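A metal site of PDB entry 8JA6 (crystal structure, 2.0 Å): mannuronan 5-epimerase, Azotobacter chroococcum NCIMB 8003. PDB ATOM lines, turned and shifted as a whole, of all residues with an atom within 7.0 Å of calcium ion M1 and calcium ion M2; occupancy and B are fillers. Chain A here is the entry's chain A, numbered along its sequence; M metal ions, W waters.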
ATOM      1  N   ASN A 322      17.228 -15.126  -1.761  1.00  0.00           N
ATOM      2  CA  ASN A 322      17.735 -13.809  -2.161  1.00  0.00           C
ATOM      3  C   ASN A 322      16.606 -12.879  -2.617  1.00  0.00           C
ATOM      4  O   ASN A 322      16.627 -12.316  -3.716  1.00  0.00           O
ATOM      5  CB  ASN A 322      18.793 -13.964  -3.239  1.00  0.00           C
ATOM      6  CG  ASN A 322      19.963 -14.774  -2.740  1.00  0.00           C
ATOM      7  OD1 ASN A 322      20.571 -14.438  -1.722  1.00  0.00           O
ATOM      8  ND2 ASN A 322      20.284 -15.874  -3.440  1.00  0.00           N
ATOM      9  N   SER A 338      11.285 -16.879   2.672  1.00  0.00           N
ATOM     10  CA  SER A 338      12.515 -17.151   1.937  1.00  0.00           C
ATOM     11  C   SER A 338      13.408 -18.066   2.770  1.00  0.00           C
ATOM     12  O   SER A 338      13.021 -18.562   3.837  1.00  0.00           O
ATOM     13  CB  SER A 338      13.207 -15.836   1.564  1.00  0.00           C
ATOM     14  OG  SER A 338      14.207 -16.050   0.582  1.00  0.00           O
ATOM     15  N   SER A 339      14.644 -18.248   2.329  1.00  0.00           N
ATOM     16  CA  SER A 339      15.510 -19.274   2.908  1.00  0.00           C
ATOM     17  C   SER A 339      16.958 -18.790   2.926  1.00  0.00           C
ATOM     18  O   SER A 339      17.192 -17.591   3.127  1.00  0.00           O
ATOM     19  CB  SER A 339      15.370 -20.595   2.161  1.00  0.00           C
ATOM     20  OG  SER A 339      16.147 -21.572   2.820  1.00  0.00           O
ATOM     21  N   GLU A 340      17.928 -19.717   2.862  1.00  0.00           N
ATOM     22  CA  GLU A 340      19.335 -19.384   3.129  1.00  0.00           C
ATOM     23  C   GLU A 340      19.781 -18.130   2.388  1.00  0.00           C
ATOM     24  O   GLU A 340      19.504 -17.961   1.190  1.00  0.00           O
ATOM     25  CB  GLU A 340      20.257 -20.552   2.746  1.00  0.00           C
ATOM     26  CG  GLU A 340      21.741 -20.153   2.971  1.00  0.00           C
ATOM     27  CD  GLU A 340      22.063 -19.974   4.478  1.00  0.00           C
ATOM     28  OE1 GLU A 340      22.241 -18.811   4.968  1.00  0.00           O
ATOM     29  OE2 GLU A 340      22.157 -21.022   5.162  1.00  0.00           O
ATOM     30  N   GLY A 341      20.464 -17.244   3.106  1.00  0.00           N
ATOM     31  CA  GLY A 341      20.954 -15.982   2.570  1.00  0.00           C
ATOM     32  C   GLY A 341      20.164 -14.805   3.112  1.00  0.00           C
ATOM     33  O   GLY A 341      19.196 -14.962   3.853  1.00  0.00           O
ATOM     34  N   ARG A 342      20.595 -13.616   2.721  1.00  0.00           N
ATOM     35  CA  ARG A 342      20.048 -12.384   3.287  1.00  0.00           C
ATOM     36  C   ARG A 342      18.807 -11.978   2.512  1.00  0.00           C
ATOM     37  O   ARG A 342      18.877 -11.730   1.307  1.00  0.00           O
ATOM     38  CB  ARG A 342      21.092 -11.264   3.264  1.00  0.00           C
ATOM     39  CG  ARG A 342      20.521  -9.889   3.675  1.00  0.00           C
ATOM     40  CD  ARG A 342      21.512  -9.181   4.601  1.00  0.00           C
ATOM     41  NE  ARG A 342      21.089  -7.814   4.896  1.00  0.00           N
ATOM     42  CZ  ARG A 342      20.172  -7.503   5.810  1.00  0.00           C
ATOM     43  NH1 ARG A 342      19.536  -8.441   6.502  1.00  0.00           N
ATOM     44  NH2 ARG A 342      19.878  -6.223   6.029  1.00  0.00           N
ATOM     45  N   ASP A 343      17.678 -11.878   3.208  1.00  0.00           N
ATOM     46  CA  ASP A 343      16.425 -11.395   2.640  1.00  0.00           C
ATOM     47  C   ASP A 343      15.990 -10.099   3.298  1.00  0.00           C
ATOM     48  O   ASP A 343      16.138  -9.932   4.511  1.00  0.00           O
ATOM     49  CB  ASP A 343      15.340 -12.461   2.803  1.00  0.00           C
ATOM     50  CG  ASP A 343      15.719 -13.745   2.101  1.00  0.00           C
ATOM     51  OD1 ASP A 343      15.536 -13.813   0.862  1.00  0.00           O
ATOM     52  OD2 ASP A 343      16.252 -14.643   2.767  1.00  0.00           O
ATOM     53  N   LEU A 345      12.538  -8.192   3.633  1.00  0.00           N
ATOM     54  CA  LEU A 345      11.120  -8.492   3.433  1.00  0.00           C
ATOM     55  C   LEU A 345      10.287  -7.442   4.151  1.00  0.00           C
ATOM     56  O   LEU A 345      10.262  -7.400   5.390  1.00  0.00           O
ATOM     57  CB  LEU A 345      10.796  -9.903   3.926  1.00  0.00           C
ATOM     58  CG  LEU A 345      11.648 -11.036   3.326  1.00  0.00           C
ATOM     59  CD1 LEU A 345      11.398 -12.364   4.013  1.00  0.00           C
ATOM     60  CD2 LEU A 345      11.433 -11.188   1.812  1.00  0.00           C
ATOM     61  N   ASP A 355       8.901 -14.561   7.012  1.00  0.00           N
ATOM     62  CA  ASP A 355       9.880 -15.529   7.511  1.00  0.00           C
ATOM     63  C   ASP A 355      11.035 -15.539   6.535  1.00  0.00           C
ATOM     64  O   ASP A 355      10.910 -16.092   5.435  1.00  0.00           O
ATOM     65  CB  ASP A 355       9.276 -16.921   7.670  1.00  0.00           C
ATOM     66  CG  ASP A 355      10.254 -17.921   8.325  1.00  0.00           C
ATOM     67  OD1 ASP A 355      11.451 -17.604   8.474  1.00  0.00           O
ATOM     68  OD2 ASP A 355       9.796 -19.023   8.708  1.00  0.00           O
ATOM     69  N   GLY A 356      12.166 -14.976   6.933  1.00  0.00           N
ATOM     70  CA  GLY A 356      13.304 -15.023   6.036  1.00  0.00           C
ATOM     71  C   GLY A 356      14.110 -16.309   6.074  1.00  0.00           C
ATOM     72  O   GLY A 356      15.078 -16.415   5.305  1.00  0.00           O
ATOM     73  N   GLY A 357      13.768 -17.272   6.936  1.00  0.00           N
ATOM     74  CA  GLY A 357      14.496 -18.543   6.941  1.00  0.00           C
ATOM     75  C   GLY A 357      15.951 -18.371   7.392  1.00  0.00           C
ATOM     76  O   GLY A 357      16.291 -17.465   8.155  1.00  0.00           O
ATOM     77  N   ALA A 358      16.820 -19.262   6.925  1.00  0.00           N
ATOM     78  CA  ALA A 358      18.227 -19.177   7.299  1.00  0.00           C
ATOM     79  C   ALA A 358      18.847 -17.859   6.820  1.00  0.00           C
ATOM     80  O   ALA A 358      18.298 -17.156   5.956  1.00  0.00           O
ATOM     81  CB  ALA A 358      19.014 -20.376   6.748  1.00  0.00           C
ATOM     82  N   GLY A 359      19.968 -17.498   7.436  1.00  0.00           N
ATOM     83  CA  GLY A 359      20.669 -16.282   7.077  1.00  0.00           C
ATOM     84  C   GLY A 359      20.098 -15.073   7.796  1.00  0.00           C
ATOM     85  O   GLY A 359      19.063 -15.133   8.482  1.00  0.00           O
ATOM     86  N   ARG A 360      20.766 -13.936   7.607  1.00  0.00           N
ATOM     87  CA  ARG A 360      20.438 -12.709   8.335  1.00  0.00           C
ATOM     88  C   ARG A 360      19.438 -11.897   7.524  1.00  0.00           C
ATOM     89  O   ARG A 360      19.780 -11.345   6.468  1.00  0.00           O
ATOM     90  CB  ARG A 360      21.695 -11.889   8.610  1.00  0.00           C
ATOM     91  CG  ARG A 360      21.370 -10.582   9.346  1.00  0.00           C
ATOM     92  CD  ARG A 360      22.606  -9.797   9.662  1.00  0.00           C
ATOM     93  NE  ARG A 360      23.057  -9.024   8.516  1.00  0.00           N
ATOM     94  CZ  ARG A 360      22.666  -7.786   8.247  1.00  0.00           C
ATOM     95  NH1 ARG A 360      21.751  -7.179   8.988  1.00  0.00           N
ATOM     96  NH2 ARG A 360      23.193  -7.147   7.202  1.00  0.00           N
ATOM     97  N   ASP A 361      18.205 -11.820   8.022  1.00  0.00           N
ATOM     98  CA  ASP A 361      17.123 -11.163   7.324  1.00  0.00           C
ATOM     99  C   ASP A 361      16.707  -9.899   8.068  1.00  0.00           C
ATOM    100  O   ASP A 361      16.819  -9.813   9.289  1.00  0.00           O
ATOM    101  CB  ASP A 361      15.936 -12.110   7.192  1.00  0.00           C
ATOM    102  CG  ASP A 361      16.382 -13.472   6.713  1.00  0.00           C
ATOM    103  OD1 ASP A 361      16.986 -13.522   5.618  1.00  0.00           O
ATOM    104  OD2 ASP A 361      16.178 -14.478   7.416  1.00  0.00           O
ATOM    105  N   THR A 362      16.204  -8.930   7.312  1.00  0.00           N
ATOM    106  CA  THR A 362      15.619  -7.717   7.875  1.00  0.00           C
ATOM    107  C   THR A 362      14.158  -7.690   7.495  1.00  0.00           C
ATOM    108  O   THR A 362      13.827  -7.712   6.295  1.00  0.00           O
ATOM    109  CB  THR A 362      16.353  -6.461   7.376  1.00  0.00           C
ATOM    110  OG1 THR A 362      17.726  -6.527   7.785  1.00  0.00           O
ATOM    111  CG2 THR A 362      15.723  -5.217   7.977  1.00  0.00           C
ATOM    112  N   LEU A 363      13.276  -7.669   8.497  1.00  0.00           N
ATOM    113  CA  LEU A 363      11.841  -7.819   8.282  1.00  0.00           C
ATOM    114  C   LEU A 363      11.091  -6.577   8.764  1.00  0.00           C
ATOM    115  O   LEU A 363      11.440  -5.993   9.803  1.00  0.00           O
ATOM    116  CB  LEU A 363      11.298  -9.046   9.012  1.00  0.00           C
ATOM    117  CG  LEU A 363      12.186 -10.306   8.939  1.00  0.00           C
ATOM    118  CD1 LEU A 363      11.835 -11.322  10.002  1.00  0.00           C
ATOM    119  CD2 LEU A 363      12.033 -10.907   7.570  1.00  0.00           C
ATOM    120  N   PHE A 374       9.747 -17.515  13.055  1.00  0.00           N
ATOM    121  CA  PHE A 374      11.094 -18.049  13.167  1.00  0.00           C
ATOM    122  C   PHE A 374      10.954 -19.555  13.293  1.00  0.00           C
ATOM    123  O   PHE A 374      10.548 -20.058  14.351  1.00  0.00           O
ATOM    124  CB  PHE A 374      11.841 -17.391  14.330  1.00  0.00           C
ATOM    125  CG  PHE A 374      12.042 -15.938  14.132  1.00  0.00           C
ATOM    126  CD1 PHE A 374      13.223 -15.454  13.609  1.00  0.00           C
ATOM    127  CD2 PHE A 374      11.020 -15.038  14.403  1.00  0.00           C
ATOM    128  CE1 PHE A 374      13.391 -14.098  13.367  1.00  0.00           C
ATOM    129  CE2 PHE A 374      11.164 -13.701  14.164  1.00  0.00           C
ATOM    130  CZ  PHE A 374      12.363 -13.224  13.651  1.00  0.00           C
ATOM    131  N   GLN A 378      18.304 -22.071  14.281  1.00  0.00           N
ATOM    132  CA  GLN A 378      19.474 -21.708  13.490  1.00  0.00           C
ATOM    133  C   GLN A 378      19.175 -20.646  12.433  1.00  0.00           C
ATOM    134  O   GLN A 378      20.072 -20.319  11.644  1.00  0.00           O
ATOM    135  CB  GLN A 378      20.052 -22.967  12.818  1.00  0.00           C
ATOM    136  CG  GLN A 378      20.986 -23.768  13.708  1.00  0.00           C
ATOM    137  CD  GLN A 378      22.252 -23.004  14.090  1.00  0.00           C
ATOM    138  OE1 GLN A 378      22.381 -22.504  15.215  1.00  0.00           O
ATOM    139  NE2 GLN A 378      23.203 -22.941  13.153  1.00  0.00           N
ATOM    140  N   ASP A 379      17.950 -20.115  12.362  1.00  0.00           N
ATOM    141  CA  ASP A 379      17.640 -19.091  11.376  1.00  0.00           C
ATOM    142  C   ASP A 379      17.933 -17.670  11.874  1.00  0.00           C
ATOM    143  O   ASP A 379      17.918 -16.734  11.070  1.00  0.00           O
ATOM    144  CB  ASP A 379      16.171 -19.200  10.951  1.00  0.00           C
ATOM    145  CG  ASP A 379      15.882 -20.490  10.154  1.00  0.00           C
ATOM    146  OD1 ASP A 379      16.832 -21.214   9.775  1.00  0.00           O
ATOM    147  OD2 ASP A 379      14.682 -20.758   9.902  1.00  0.00           O
ATOM    148  N   SER A 380      18.226 -17.496  13.161  1.00  0.00           N
ATOM    149  CA  SER A 380      18.558 -16.176  13.722  1.00  0.00           C
ATOM    150  C   SER A 380      19.349 -16.439  14.990  1.00  0.00           C
ATOM    151  O   SER A 380      18.773 -16.911  15.976  1.00  0.00           O
ATOM    152  CB  SER A 380      17.287 -15.377  13.998  1.00  0.00           C
ATOM    153  OG  SER A 380      17.557 -14.025  14.371  1.00  0.00           O
ATOM    154  N   PHE A 381      20.663 -16.181  14.961  1.00  0.00           N
ATOM    155  CA  PHE A 381      21.499 -16.571  16.083  1.00  0.00           C
ATOM    156  C   PHE A 381      22.792 -15.760  16.137  1.00  0.00           C
ATOM    157  O   PHE A 381      23.260 -15.219  15.127  1.00  0.00           O
ATOM    158  CB  PHE A 381      21.836 -18.063  16.043  1.00  0.00           C
ATOM    159  CG  PHE A 381      22.777 -18.446  14.916  1.00  0.00           C
ATOM    160  CD1 PHE A 381      24.148 -18.521  15.131  1.00  0.00           C
ATOM    161  CD2 PHE A 381      22.284 -18.717  13.646  1.00  0.00           C
ATOM    162  CE1 PHE A 381      25.018 -18.868  14.108  1.00  0.00           C
ATOM    163  CE2 PHE A 381      23.139 -19.073  12.606  1.00  0.00           C
ATOM    164  CZ  PHE A 381      24.512 -19.139  12.833  1.00  0.00           C
ATOM    165  N   ARG A 390      24.559 -13.200  11.905  1.00  0.00           N
ATOM    166  CA  ARG A 390      23.427 -14.058  11.543  1.00  0.00           C
ATOM    167  C   ARG A 390      22.196 -13.780  12.403  1.00  0.00           C
ATOM    168  O   ARG A 390      21.283 -14.625  12.462  1.00  0.00           O
ATOM    169  CB  ARG A 390      23.822 -15.542  11.623  1.00  0.00           C
ATOM    170  CG  ARG A 390      25.063 -15.905  10.821  1.00  0.00           C
ATOM    171  CD  ARG A 390      24.841 -16.040   9.322  1.00  0.00           C
ATOM    172  NE  ARG A 390      23.898 -17.095   8.950  1.00  0.00           N
ATOM    173  CZ  ARG A 390      24.222 -18.319   8.551  1.00  0.00           C
ATOM    174  NH1 ARG A 390      25.483 -18.744   8.585  1.00  0.00           N
ATOM    175  NH2 ARG A 390      23.260 -19.132   8.109  1.00  0.00           N
ATOM    176  N   VAL A 391      22.115 -12.614  13.054  1.00  0.00           N
ATOM    177  CA  VAL A 391      20.950 -12.237  13.848  1.00  0.00           C
ATOM    178  C   VAL A 391      19.989 -11.431  12.978  1.00  0.00           C
ATOM    179  O   VAL A 391      20.359 -10.362  12.475  1.00  0.00           O
ATOM    180  CB  VAL A 391      21.346 -11.451  15.101  1.00  0.00           C
ATOM    181  CG1 VAL A 391      20.101 -10.996  15.849  1.00  0.00           C
ATOM    182  CG2 VAL A 391      22.268 -12.272  15.999  1.00  0.00           C
ATOM    183  N   ASP A 392      18.751 -11.923  12.831  1.00  0.00           N
ATOM    184  CA  ASP A 392      17.692 -11.179  12.151  1.00  0.00           C
ATOM    185  C   ASP A 392      17.278  -9.944  12.936  1.00  0.00           C
ATOM    186  O   ASP A 392      17.309  -9.928  14.175  1.00  0.00           O
ATOM    187  CB  ASP A 392      16.425 -12.034  11.971  1.00  0.00           C
ATOM    188  CG  ASP A 392      16.571 -13.115  10.935  1.00  0.00           C
ATOM    189  OD1 ASP A 392      17.666 -13.326  10.381  1.00  0.00           O
ATOM    190  OD2 ASP A 392      15.532 -13.770  10.684  1.00  0.00           O
HETATM  191 CA    CA M   1      16.823 -15.516   9.383  1.00  0.00          CA
HETATM  192 CA    CA M   2      17.164 -15.696   4.635  1.00  0.00          CA
HETATM  193  O   HOH W   1      14.607 -16.284  10.396  1.00  0.00           O
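The backbone NH (N) of Ala 358 lies within hydrogen-bond range of the side-chain carboxylate (OD1) of Asp 379, 3.5 Å away. OD1 of Asp 343 lies within hydrogen-bond range of OG of Ser 338, at 2.6 Å. N of Asn 322 sits at hydrogen-bond distance from OD1 of Asp 343, 3.4 Å away. O of Asp 343 lies within hydrogen-bond range of N of Thr 362, 3.0 Å away. The backbone NH of Gly 357 lies close to the backbone carbonyl oxygen of Ser 338, 3.4 Å away. N of Gly 357 lies within hydrogen-bond range of OD1 of Asp 355, at 2.8 Å. The backbone NH (N) of Asp 392 is in hydrogen-bond range of the side-chain hydroxyl (OG) of Ser 380 (2.9 Å).
Of the 25 residues printed, 6 come within 4 Å of calcium ion M2.
Calcium ion M1 is bound by the side-chain carboxylate (OD2) of Asp 361, the backbone carbonyl oxygen (O) of Asp 379, the backbone carbonyl oxygen (O) of Gly 357, the backbone carbonyl oxygen (O) of Gly 359, the side-chain carboxylate (OD2) of Asp 392, the side-chain carboxylate (OD1) of Asp 392 and water W1.
Of the 25 residues printed, 5 come within 4 Å of calcium ion M1. Along chain A the residues within 4 Å of calcium ion M1 span positions 357 to 392.
Calcium ion M2 is bound by O of Ala 358 (2.3 Å). The backbone carbonyl oxygen (O) of Gly 341 binds calcium ion M2 (2.3 Å). The backbone carbonyl oxygen (O) of Gly 356 is bound to calcium ion M2. Calcium ion M2 is bound by OD2 of Asp 343 (2.3 Å). Calcium ion M2 is bound by OD1 of Asp 361, 2.4 Å away. O of Ser 339 binds calcium ion M2 (2.4 Å). Calcium ion M2 has six donor atoms within binding distance.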
